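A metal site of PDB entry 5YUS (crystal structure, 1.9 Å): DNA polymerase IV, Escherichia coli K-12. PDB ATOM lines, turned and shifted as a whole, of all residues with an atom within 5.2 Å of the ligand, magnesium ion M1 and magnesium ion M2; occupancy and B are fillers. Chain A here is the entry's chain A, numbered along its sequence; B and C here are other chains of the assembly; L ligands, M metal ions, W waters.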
ATOM      1  N   ASP A   9     -12.432  19.082  13.199  1.00  0.00           N
ATOM      2  CA  ASP A   9     -12.258  19.330  11.764  1.00  0.00           C
ATOM      3  C   ASP A   9     -11.911  18.016  11.094  1.00  0.00           C
ATOM      4  O   ASP A   9     -10.933  17.375  11.465  1.00  0.00           O
ATOM      5  CB  ASP A   9     -11.151  20.373  11.544  1.00  0.00           C
ATOM      6  CG  ASP A   9     -11.005  20.777  10.074  1.00  0.00           C
ATOM      7  OD1 ASP A   9     -10.471  19.995   9.267  1.00  0.00           O
ATOM      8  OD2 ASP A   9     -11.403  21.906   9.730  1.00  0.00           O
ATOM      9  N   MET A  10     -12.704  17.593  10.112  1.00  0.00           N
ATOM     10  CA  MET A  10     -12.390  16.331   9.441  1.00  0.00           C
ATOM     11  C   MET A  10     -11.137  16.488   8.579  1.00  0.00           C
ATOM     12  O   MET A  10     -10.898  17.538   7.995  1.00  0.00           O
ATOM     13  CB  MET A  10     -13.562  15.876   8.563  1.00  0.00           C
ATOM     14  CG  MET A  10     -14.873  15.678   9.298  1.00  0.00           C
ATOM     15  SD  MET A  10     -14.726  14.371  10.519  1.00  0.00           S
ATOM     16  CE  MET A  10     -14.389  12.974   9.438  1.00  0.00           C
ATOM     17  N   ASP A  11     -10.345  15.424   8.489  1.00  0.00           N
ATOM     18  CA  ASP A  11      -9.134  15.437   7.664  1.00  0.00           C
ATOM     19  C   ASP A  11      -9.476  15.147   6.206  1.00  0.00           C
ATOM     20  O   ASP A  11     -10.165  14.157   5.910  1.00  0.00           O
ATOM     21  CB  ASP A  11      -8.106  14.420   8.166  1.00  0.00           C
ATOM     22  CG  ASP A  11      -7.751  14.595   9.635  1.00  0.00           C
ATOM     23  OD1 ASP A  11      -7.458  15.730  10.041  1.00  0.00           O
ATOM     24  OD2 ASP A  11      -7.765  13.591  10.381  1.00  0.00           O
ATOM     25  N   CYS A  12      -9.002  16.009   5.297  1.00  0.00           N
ATOM     26  CA  CYS A  12      -9.157  15.898   3.835  1.00  0.00           C
ATOM     27  C   CYS A  12     -10.549  15.401   3.443  1.00  0.00           C
ATOM     28  O   CYS A  12     -10.713  14.440   2.706  1.00  0.00           O
ATOM     29  CB  CYS A  12      -8.089  14.978   3.245  1.00  0.00           C
ATOM     30  SG  CYS A  12      -6.420  15.552   3.514  1.00  0.00           S
ATOM     31  N   PHE A  13     -11.550  16.142   3.932  1.00  0.00           N
ATOM     32  CA  PHE A  13     -12.892  15.581   4.110  1.00  0.00           C
ATOM     33  C   PHE A  13     -13.401  14.865   2.867  1.00  0.00           C
ATOM     34  O   PHE A  13     -13.657  13.656   2.906  1.00  0.00           O
ATOM     35  CB  PHE A  13     -13.872  16.675   4.551  1.00  0.00           C
ATOM     36  CG  PHE A  13     -15.249  16.172   4.812  1.00  0.00           C
ATOM     37  CD1 PHE A  13     -15.442  14.991   5.527  1.00  0.00           C
ATOM     38  CD2 PHE A  13     -16.357  16.869   4.355  1.00  0.00           C
ATOM     39  CE1 PHE A  13     -16.719  14.509   5.758  1.00  0.00           C
ATOM     40  CE2 PHE A  13     -17.644  16.404   4.596  1.00  0.00           C
ATOM     41  CZ  PHE A  13     -17.829  15.218   5.308  1.00  0.00           C
ATOM     42  N   PHE A  14     -13.566  15.587   1.746  1.00  0.00           N
ATOM     43  CA  PHE A  14     -14.132  14.966   0.552  1.00  0.00           C
ATOM     44  C   PHE A  14     -13.259  13.805   0.088  1.00  0.00           C
ATOM     45  O   PHE A  14     -13.772  12.751  -0.287  1.00  0.00           O
ATOM     46  CB  PHE A  14     -14.292  15.961  -0.605  1.00  0.00           C
ATOM     47  CG  PHE A  14     -15.352  17.006  -0.391  1.00  0.00           C
ATOM     48  CD1 PHE A  14     -16.067  17.093   0.784  1.00  0.00           C
ATOM     49  CD2 PHE A  14     -15.657  17.899  -1.417  1.00  0.00           C
ATOM     50  CE1 PHE A  14     -17.027  18.057   0.965  1.00  0.00           C
ATOM     51  CE2 PHE A  14     -16.620  18.858  -1.259  1.00  0.00           C
ATOM     52  CZ  PHE A  14     -17.310  18.948  -0.067  1.00  0.00           C
ATOM     53  N   ALA A  15     -11.944  14.000   0.077  1.00  0.00           N
ATOM     54  CA  ALA A  15     -11.045  12.947  -0.389  1.00  0.00           C
ATOM     55  C   ALA A  15     -11.015  11.765   0.581  1.00  0.00           C
ATOM     56  O   ALA A  15     -10.848  10.621   0.143  1.00  0.00           O
ATOM     57  CB  ALA A  15      -9.631  13.498  -0.593  1.00  0.00           C
ATOM     58  N   ILE A  42      -9.716  22.719  -7.973  1.00  0.00           N
ATOM     59  CA  ILE A  42      -9.643  21.653  -6.984  1.00  0.00           C
ATOM     60  C   ILE A  42     -10.465  22.051  -5.761  1.00  0.00           C
ATOM     61  O   ILE A  42     -10.244  23.123  -5.182  1.00  0.00           O
ATOM     62  CB  ILE A  42      -8.182  21.377  -6.570  1.00  0.00           C
ATOM     63  CG1 ILE A  42      -7.310  21.053  -7.785  1.00  0.00           C
ATOM     64  CG2 ILE A  42      -8.105  20.272  -5.487  1.00  0.00           C
ATOM     65  CD1 ILE A  42      -7.818  19.889  -8.609  1.00  0.00           C
ATOM     66  N   SER A  43     -11.400  21.177  -5.353  1.00  0.00           N
ATOM     67  CA  SER A  43     -12.063  21.349  -4.063  1.00  0.00           C
ATOM     68  C   SER A  43     -11.168  20.901  -2.920  1.00  0.00           C
ATOM     69  O   SER A  43     -11.028  21.595  -1.912  1.00  0.00           O
ATOM     70  CB  SER A  43     -13.386  20.582  -4.041  1.00  0.00           C
ATOM     71  OG  SER A  43     -14.446  21.373  -4.559  1.00  0.00           O
ATOM     72  N   THR A  44     -10.564  19.721  -3.054  1.00  0.00           N
ATOM     73  CA  THR A  44      -9.604  19.261  -2.060  1.00  0.00           C
ATOM     74  C   THR A  44      -8.813  18.103  -2.648  1.00  0.00           C
ATOM     75  O   THR A  44      -9.152  17.568  -3.696  1.00  0.00           O
ATOM     76  CB  THR A  44     -10.302  18.855  -0.754  1.00  0.00           C
ATOM     77  OG1 THR A  44      -9.335  18.648   0.276  1.00  0.00           O
ATOM     78  CG2 THR A  44     -11.102  17.571  -0.971  1.00  0.00           C
ATOM     79  N   TYR A  47      -3.332  13.439   0.768  1.00  0.00           N
ATOM     80  CA  TYR A  47      -1.956  13.788   1.085  1.00  0.00           C
ATOM     81  C   TYR A  47      -0.967  13.398  -0.012  1.00  0.00           C
ATOM     82  O   TYR A  47       0.013  14.110  -0.212  1.00  0.00           O
ATOM     83  CB  TYR A  47      -1.548  13.174   2.426  1.00  0.00           C
ATOM     84  CG  TYR A  47      -1.979  14.064   3.572  1.00  0.00           C
ATOM     85  CD1 TYR A  47      -1.237  15.199   3.896  1.00  0.00           C
ATOM     86  CD2 TYR A  47      -3.136  13.809   4.271  1.00  0.00           C
ATOM     87  CE1 TYR A  47      -1.635  16.042   4.920  1.00  0.00           C
ATOM     88  CE2 TYR A  47      -3.548  14.649   5.298  1.00  0.00           C
ATOM     89  CZ  TYR A  47      -2.794  15.763   5.620  1.00  0.00           C
ATOM     90  OH  TYR A  47      -3.197  16.586   6.636  1.00  0.00           O
ATOM     91  N   ARG A  50      -1.162  16.334  -2.196  1.00  0.00           N
ATOM     92  CA  ARG A  50      -0.639  17.545  -1.559  1.00  0.00           C
ATOM     93  C   ARG A  50       0.889  17.597  -1.593  1.00  0.00           C
ATOM     94  O   ARG A  50       1.463  18.687  -1.606  1.00  0.00           O
ATOM     95  CB  ARG A  50      -1.139  17.636  -0.125  1.00  0.00           C
ATOM     96  CG  ARG A  50      -2.630  17.877  -0.046  1.00  0.00           C
ATOM     97  CD  ARG A  50      -3.161  18.075   1.355  1.00  0.00           C
ATOM     98  NE  ARG A  50      -4.614  18.172   1.334  1.00  0.00           N
ATOM     99  CZ  ARG A  50      -5.360  18.662   2.316  1.00  0.00           C
ATOM    100  NH1 ARG A  50      -4.789  19.104   3.438  1.00  0.00           N
ATOM    101  NH2 ARG A  50      -6.680  18.698   2.184  1.00  0.00           N
ATOM    102  N   SER A  56      -6.424  23.040  -2.323  1.00  0.00           N
ATOM    103  CA  SER A  56      -7.750  23.577  -2.552  1.00  0.00           C
ATOM    104  C   SER A  56      -7.681  24.906  -3.278  1.00  0.00           C
ATOM    105  O   SER A  56      -6.780  25.716  -3.058  1.00  0.00           O
ATOM    106  CB  SER A  56      -8.481  23.755  -1.229  1.00  0.00           C
ATOM    107  OG  SER A  56      -8.812  22.511  -0.662  1.00  0.00           O
ATOM    108  N   ALA A  57      -8.654  25.120  -4.166  1.00  0.00           N
ATOM    109  CA  ALA A  57      -8.850  26.343  -4.946  1.00  0.00           C
ATOM    110  C   ALA A  57      -7.823  26.489  -6.056  1.00  0.00           C
ATOM    111  O   ALA A  57      -7.927  27.419  -6.860  1.00  0.00           O
ATOM    112  CB  ALA A  57      -8.848  27.608  -4.067  1.00  0.00           C
ATOM    113  N   SER A 102     -19.309  24.362   8.724  1.00  0.00           N
ATOM    114  CA  SER A 102     -19.326  23.798   7.377  1.00  0.00           C
ATOM    115  C   SER A 102     -19.771  22.364   7.559  1.00  0.00           C
ATOM    116  O   SER A 102     -20.030  21.927   8.681  1.00  0.00           O
ATOM    117  CB  SER A 102     -17.952  23.866   6.712  1.00  0.00           C
ATOM    118  OG  SER A 102     -17.022  23.032   7.395  1.00  0.00           O
ATOM    119  N   ASP A 104     -17.912  19.864   7.574  1.00  0.00           N
ATOM    120  CA  ASP A 104     -16.891  19.018   8.179  1.00  0.00           C
ATOM    121  C   ASP A 104     -16.289  19.604   9.450  1.00  0.00           C
ATOM    122  O   ASP A 104     -15.318  19.046   9.975  1.00  0.00           O
ATOM    123  CB  ASP A 104     -15.790  18.715   7.160  1.00  0.00           C
ATOM    124  CG  ASP A 104     -14.608  19.702   7.200  1.00  0.00           C
ATOM    125  OD1 ASP A 104     -14.797  20.926   7.329  1.00  0.00           O
ATOM    126  OD2 ASP A 104     -13.463  19.243   7.096  1.00  0.00           O
ATOM    127  N   GLU A 105     -16.822  20.711   9.975  1.00  0.00           N
ATOM    128  CA  GLU A 105     -16.237  21.216  11.213  1.00  0.00           C
ATOM    129  C   GLU A 105     -17.288  21.907  12.057  1.00  0.00           C
ATOM    130  O   GLU A 105     -18.320  22.365  11.559  1.00  0.00           O
ATOM    131  CB  GLU A 105     -15.054  22.150  10.944  1.00  0.00           C
ATOM    132  CG  GLU A 105     -15.338  23.285  10.013  1.00  0.00           C
ATOM    133  CD  GLU A 105     -14.096  24.120   9.705  1.00  0.00           C
ATOM    134  OE1 GLU A 105     -13.835  25.098  10.434  1.00  0.00           O
ATOM    135  OE2 GLU A 105     -13.375  23.784   8.743  1.00  0.00           O
ATOM    136  N   LYS A 151      -9.505  26.673  16.937  1.00  0.00           N
ATOM    137  CA  LYS A 151      -9.391  26.466  15.502  1.00  0.00           C
ATOM    138  C   LYS A 151      -7.930  26.309  15.072  1.00  0.00           C
ATOM    139  O   LYS A 151      -7.566  25.342  14.398  1.00  0.00           O
ATOM    140  CB  LYS A 151     -10.072  27.634  14.778  1.00  0.00           C
ATOM    141  CG  LYS A 151      -9.872  27.711  13.278  1.00  0.00           C
ATOM    142  CD  LYS A 151     -10.430  26.512  12.543  1.00  0.00           C
ATOM    143  CE  LYS A 151     -10.371  26.749  11.032  1.00  0.00           C
ATOM    144  NZ  LYS A 151     -10.593  25.497  10.257  1.00  0.00           N
ATOM    145  N   ASP A 155      -5.386  22.492  13.752  1.00  0.00           N
ATOM    146  CA  ASP A 155      -4.501  22.267  12.614  1.00  0.00           C
ATOM    147  C   ASP A 155      -3.113  21.783  13.009  1.00  0.00           C
ATOM    148  O   ASP A 155      -2.361  21.324  12.142  1.00  0.00           O
ATOM    149  CB  ASP A 155      -4.358  23.551  11.789  1.00  0.00           C
ATOM    150  CG  ASP A 155      -5.551  23.800  10.866  1.00  0.00           C
ATOM    151  OD1 ASP A 155      -5.980  22.868  10.160  1.00  0.00           O
ATOM    152  OD2 ASP A 155      -6.047  24.944  10.863  1.00  0.00           O
ATOM    153  N   LYS A 158      -2.627  17.844  12.864  1.00  0.00           N
ATOM    154  CA  LYS A 158      -3.414  17.259  11.794  1.00  0.00           C
ATOM    155  C   LYS A 158      -2.468  16.539  10.819  1.00  0.00           C
ATOM    156  O   LYS A 158      -1.376  17.029  10.554  1.00  0.00           O
ATOM    157  CB  LYS A 158      -4.221  18.350  11.093  1.00  0.00           C
ATOM    158  CG  LYS A 158      -5.084  17.924   9.925  1.00  0.00           C
ATOM    159  CD  LYS A 158      -5.786  19.140   9.274  1.00  0.00           C
ATOM    160  CE  LYS A 158      -7.133  19.463   9.930  1.00  0.00           C
ATOM    161  NZ  LYS A 158      -8.197  18.437   9.633  1.00  0.00           N
ATOM    162  P    DA B   4     -13.138  29.742 -10.953  1.00  0.00           P
ATOM    163  OP1  DA B   4     -13.777  30.297 -12.176  1.00  0.00           O
ATOM    164  OP2  DA B   4     -12.938  30.620  -9.786  1.00  0.00           O
ATOM    165  O5'  DA B   4     -13.936  28.451 -10.469  1.00  0.00           O
ATOM    166  C5'  DA B   4     -14.138  27.322 -11.342  1.00  0.00           C
ATOM    167  C4'  DA B   4     -15.362  26.534 -10.915  1.00  0.00           C
ATOM    168  O4'  DA B   4     -15.136  25.952  -9.609  1.00  0.00           O
ATOM    169  C3'  DA B   4     -16.632  27.346 -10.771  1.00  0.00           C
ATOM    170  O3'  DA B   4     -17.778  26.530 -11.096  1.00  0.00           O
ATOM    171  C2'  DA B   4     -16.633  27.755  -9.310  1.00  0.00           C
ATOM    172  C1'  DA B   4     -15.922  26.588  -8.628  1.00  0.00           C
ATOM    173  N9   DA B   4     -15.010  27.013  -7.553  1.00  0.00           N
ATOM    174  C8   DA B   4     -14.245  28.139  -7.524  1.00  0.00           C
ATOM    175  N7   DA B   4     -13.501  28.253  -6.431  1.00  0.00           N
ATOM    176  C5   DA B   4     -13.811  27.118  -5.696  1.00  0.00           C
ATOM    177  C6   DA B   4     -13.362  26.638  -4.452  1.00  0.00           C
ATOM    178  N6   DA B   4     -12.471  27.269  -3.686  1.00  0.00           N
ATOM    179  N1   DA B   4     -13.869  25.456  -4.012  1.00  0.00           N
ATOM    180  C2   DA B   4     -14.753  24.819  -4.783  1.00  0.00           C
ATOM    181  N3   DA B   4     -15.251  25.169  -5.970  1.00  0.00           N
ATOM    182  C4   DA B   4     -14.734  26.334  -6.375  1.00  0.00           C
ATOM    183  P    DG B   5     -19.258  27.118 -11.054  1.00  0.00           P
ATOM    184  OP1  DG B   5     -20.043  26.314 -12.020  1.00  0.00           O
ATOM    185  OP2  DG B   5     -19.260  28.593 -11.169  1.00  0.00           O
ATOM    186  O5'  DG B   5     -19.745  26.865  -9.566  1.00  0.00           O
ATOM    187  C5'  DG B   5     -19.918  25.546  -9.079  1.00  0.00           C
ATOM    188  C4'  DG B   5     -20.337  25.611  -7.634  1.00  0.00           C
ATOM    189  O4'  DG B   5     -19.183  25.967  -6.819  1.00  0.00           O
ATOM    190  C3'  DG B   5     -21.418  26.651  -7.337  1.00  0.00           C
ATOM    191  O3'  DG B   5     -22.375  26.122  -6.446  1.00  0.00           O
ATOM    192  C2'  DG B   5     -20.634  27.791  -6.693  1.00  0.00           C
ATOM    193  C1'  DG B   5     -19.591  26.996  -5.945  1.00  0.00           C
ATOM    194  N9   DG B   5     -18.425  27.772  -5.520  1.00  0.00           N
ATOM    195  C8   DG B   5     -17.840  28.850  -6.144  1.00  0.00           C
ATOM    196  N7   DG B   5     -16.813  29.326  -5.476  1.00  0.00           N
ATOM    197  C5   DG B   5     -16.718  28.520  -4.363  1.00  0.00           C
ATOM    198  C6   DG B   5     -15.803  28.556  -3.275  1.00  0.00           C
ATOM    199  O6   DG B   5     -14.855  29.326  -3.087  1.00  0.00           O
ATOM    200  N1   DG B   5     -16.076  27.538  -2.348  1.00  0.00           N
ATOM    201  C2   DG B   5     -17.095  26.624  -2.458  1.00  0.00           C
ATOM    202  N2   DG B   5     -17.214  25.727  -1.461  1.00  0.00           N
ATOM    203  N3   DG B   5     -17.944  26.593  -3.459  1.00  0.00           N
ATOM    204  C4   DG B   5     -17.709  27.570  -4.360  1.00  0.00           C
ATOM    205  P    DC C  18     -12.441  27.832   7.866  1.00  0.00           P
ATOM    206  OP1  DC C  18     -12.934  27.585   9.244  1.00  0.00           O
ATOM    207  OP2  DC C  18     -10.998  27.674   7.543  1.00  0.00           O
ATOM    208  O5'  DC C  18     -13.193  26.909   6.812  1.00  0.00           O
ATOM    209  C5'  DC C  18     -14.597  26.827   6.797  1.00  0.00           C
ATOM    210  C4'  DC C  18     -15.027  25.965   5.646  1.00  0.00           C
ATOM    211  O4'  DC C  18     -15.000  26.761   4.459  1.00  0.00           O
ATOM    212  C3'  DC C  18     -14.098  24.776   5.380  1.00  0.00           C
ATOM    213  O3'  DC C  18     -14.736  23.569   5.755  1.00  0.00           O
ATOM    214  C2'  DC C  18     -13.816  24.834   3.860  1.00  0.00           C
ATOM    215  C1'  DC C  18     -14.786  25.896   3.363  1.00  0.00           C
ATOM    216  N1   DC C  18     -14.264  26.709   2.248  1.00  0.00           N
ATOM    217  C2   DC C  18     -14.906  26.654   1.018  1.00  0.00           C
ATOM    218  O2   DC C  18     -15.892  25.909   0.897  1.00  0.00           O
ATOM    219  N3   DC C  18     -14.436  27.407  -0.008  1.00  0.00           N
ATOM    220  C4   DC C  18     -13.369  28.192   0.165  1.00  0.00           C
ATOM    221  N4   DC C  18     -12.960  28.907  -0.883  1.00  0.00           N
ATOM    222  C5   DC C  18     -12.688  28.261   1.425  1.00  0.00           C
ATOM    223  C6   DC C  18     -13.169  27.509   2.432  1.00  0.00           C
HETATM  224  P1  LIG L   1     -11.266  22.008   4.735  1.00  0.00           P
HETATM  225  O1  LIG L   1     -11.479  21.537   6.159  1.00  0.00           O
HETATM  226  O2  LIG L   1     -10.752  23.424   4.719  1.00  0.00           O
HETATM  227  O3  LIG L   1     -10.197  21.095   3.955  1.00  0.00           O
HETATM  228  P2  LIG L   1     -10.021  19.502   4.115  1.00  0.00           P
HETATM  229  O4  LIG L   1     -10.116  18.849   2.750  1.00  0.00           O
HETATM  230  O5  LIG L   1     -10.967  18.847   5.070  1.00  0.00           O
HETATM  231  O6  LIG L   1      -8.468  19.390   4.465  1.00  0.00           O
HETATM  232  P3  LIG L   1      -7.852  19.502   5.956  1.00  0.00           P
HETATM  233  O7  LIG L   1      -8.840  20.159   6.903  1.00  0.00           O
HETATM  234  O8  LIG L   1      -6.615  20.339   5.866  1.00  0.00           O
HETATM  235  O9  LIG L   1      -7.485  18.125   6.423  1.00  0.00           O
HETATM  236  O10 LIG L   1     -12.536  21.852   3.773  1.00  0.00           O
HETATM  237  C1  LIG L   1     -13.562  20.873   3.999  1.00  0.00           C
HETATM  238  C2  LIG L   1     -14.105  20.444   2.636  1.00  0.00           C
HETATM  239  O11 LIG L   1     -14.693  21.566   1.966  1.00  0.00           O
HETATM  240  C3  LIG L   1     -13.017  19.939   1.698  1.00  0.00           C
HETATM  241  O12 LIG L   1     -12.743  18.549   1.877  1.00  0.00           O
HETATM  242  C4  LIG L   1     -13.596  20.270   0.320  1.00  0.00           C
HETATM  243  C5  LIG L   1     -14.413  21.532   0.564  1.00  0.00           C
HETATM  244  N1  LIG L   1     -13.611  22.711   0.164  1.00  0.00           N
HETATM  245  C6  LIG L   1     -13.850  23.290  -1.093  1.00  0.00           C
HETATM  246  O13 LIG L   1     -14.733  22.810  -1.826  1.00  0.00           O
HETATM  247  N2  LIG L   1     -13.161  24.357  -1.524  1.00  0.00           N
HETATM  248  C7  LIG L   1     -12.201  24.902  -0.772  1.00  0.00           C
HETATM  249  O14 LIG L   1     -11.561  25.882  -1.218  1.00  0.00           O
HETATM  250  C8  LIG L   1     -11.905  24.325   0.561  1.00  0.00           C
HETATM  251  C9  LIG L   1     -10.815  24.908   1.430  1.00  0.00           C
HETATM  252  C10 LIG L   1     -12.662  23.213   0.968  1.00  0.00           C
HETATM  253 MG    MG M   1     -13.159  22.110   7.865  1.00  0.00          MG
HETATM  254 MG    MG M   2     -11.187  19.659   7.178  1.00  0.00          MG
HETATM  255  O   HOH W   1      -8.581  22.503   7.910  1.00  0.00           O
HETATM  256  O   HOH W   2     -17.631  22.192  -2.438  1.00  0.00           O
HETATM  257  O   HOH W   3     -11.100  23.839   7.954  1.00  0.00           O
HETATM  258  O   HOH W   4      -5.685  16.419   7.287  1.00  0.00           O
HETATM  259  O   HOH W   5      -9.511  27.618  -0.396  1.00  0.00           O
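OG1 of Thr 44 sits at hydrogen-bond distance from O4 of the ligand.
A nitrogen (N2) of the ligand sits at hydrogen-bond distance from N1 of DA 4 of chain B, 2.8 Å away.
N of Cys 12 sits at hydrogen-bond distance from O9 of the ligand.
An oxygen (O8) of the ligand is in salt-bridge range of the guanidinium group (NH1) of Arg 50 (3.3 Å).
The backbone NH (N) of Phe 13 sits at hydrogen-bond distance from an oxygen (O4) of the ligand, 3.3 Å away.
O12 of the ligand is in hydrogen-bond range of N of Phe 14, at 3.1 Å.
The side-chain hydroxyl of Ser 43 sits at hydrogen-bond distance from an oxygen (O13) of the ligand (3.1 Å).
An oxygen (O9) of the ligand is in salt-bridge range of the side-chain amino group of Lys 158, at 3.3 Å.
The backbone carbonyl oxygen (O) of Asp 9 sits at hydrogen-bond distance from the side-chain amino group (NZ) of Lys 158 (3.5 Å).
OD2 of Asp 9 sits close to NZ of Lys 151 (3.7 Å).
NH2 of Arg 50 sits at hydrogen-bond distance from OG1 of Thr 44 (3.3 Å).
The guanidinium group (NH2) of Arg 50 is in hydrogen-bond range of the side-chain sulfur (SG) of Cys 12 (3.4 Å).
O2 of DC 18 of chain C lies close to N2 of DG 5 of chain B, 2.7 Å away.
O3' of DC 18 of chain C sits at hydrogen-bond distance from OG of Ser 102.
OP1 of DC 18 of chain C is in salt-bridge range of NZ of Lys 151 (3.3 Å).
The backbone carbonyl oxygen of Ser 43 is in hydrogen-bond range of the side-chain hydroxyl of Ser 56 (2.7 Å).
N4 of DC 18 of chain C sits close to an oxygen (O14) of the ligand (3.3 Å).
Merely in contact with the ligand: Asp 11, Ser 56 and DG 5 of chain B.
Hydrophobic or aromatic side chains within 4 Å of the ligand: Phe 13 and Phe 14.
Of the 23 residues printed, 16 come within 4 Å of the ligand.
OG of Ser 102 touches magnesium ion M1, at 3.999 Å.
DC 18 of chain C touches magnesium ion M1.
Three residues have an atom within 4 Å of magnesium ion M2: Asp 9, Met 10 and Asp 104.
The nearest printed residue that does not touch magnesium ion M2 is Lys 158 (4.1 Å).
Magnesium ion M1 is bound by OE2 of Glu 105, OD1 of Asp 104, O1 of the ligand and OD2 of Asp 9.
Magnesium ion M1 has four donor atoms within binding distance.
Slightly farther from magnesium ion M1 lies water W3 (2.7 Å).
Magnesium ion M2 is bound by O1 of the ligand, OD1 of Asp 9, O5 of the ligand, O of Met 10, OD2 of Asp 104 and O7 of the ligand.
Water W3 bridges NZ of Lys 151 (2.9 Å) and O2 of the ligand (3.3 Å).
Water W4 lies within hydrogen-bond range of OH of Tyr 47, O9 of the ligand and OD1 of Asp 11.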
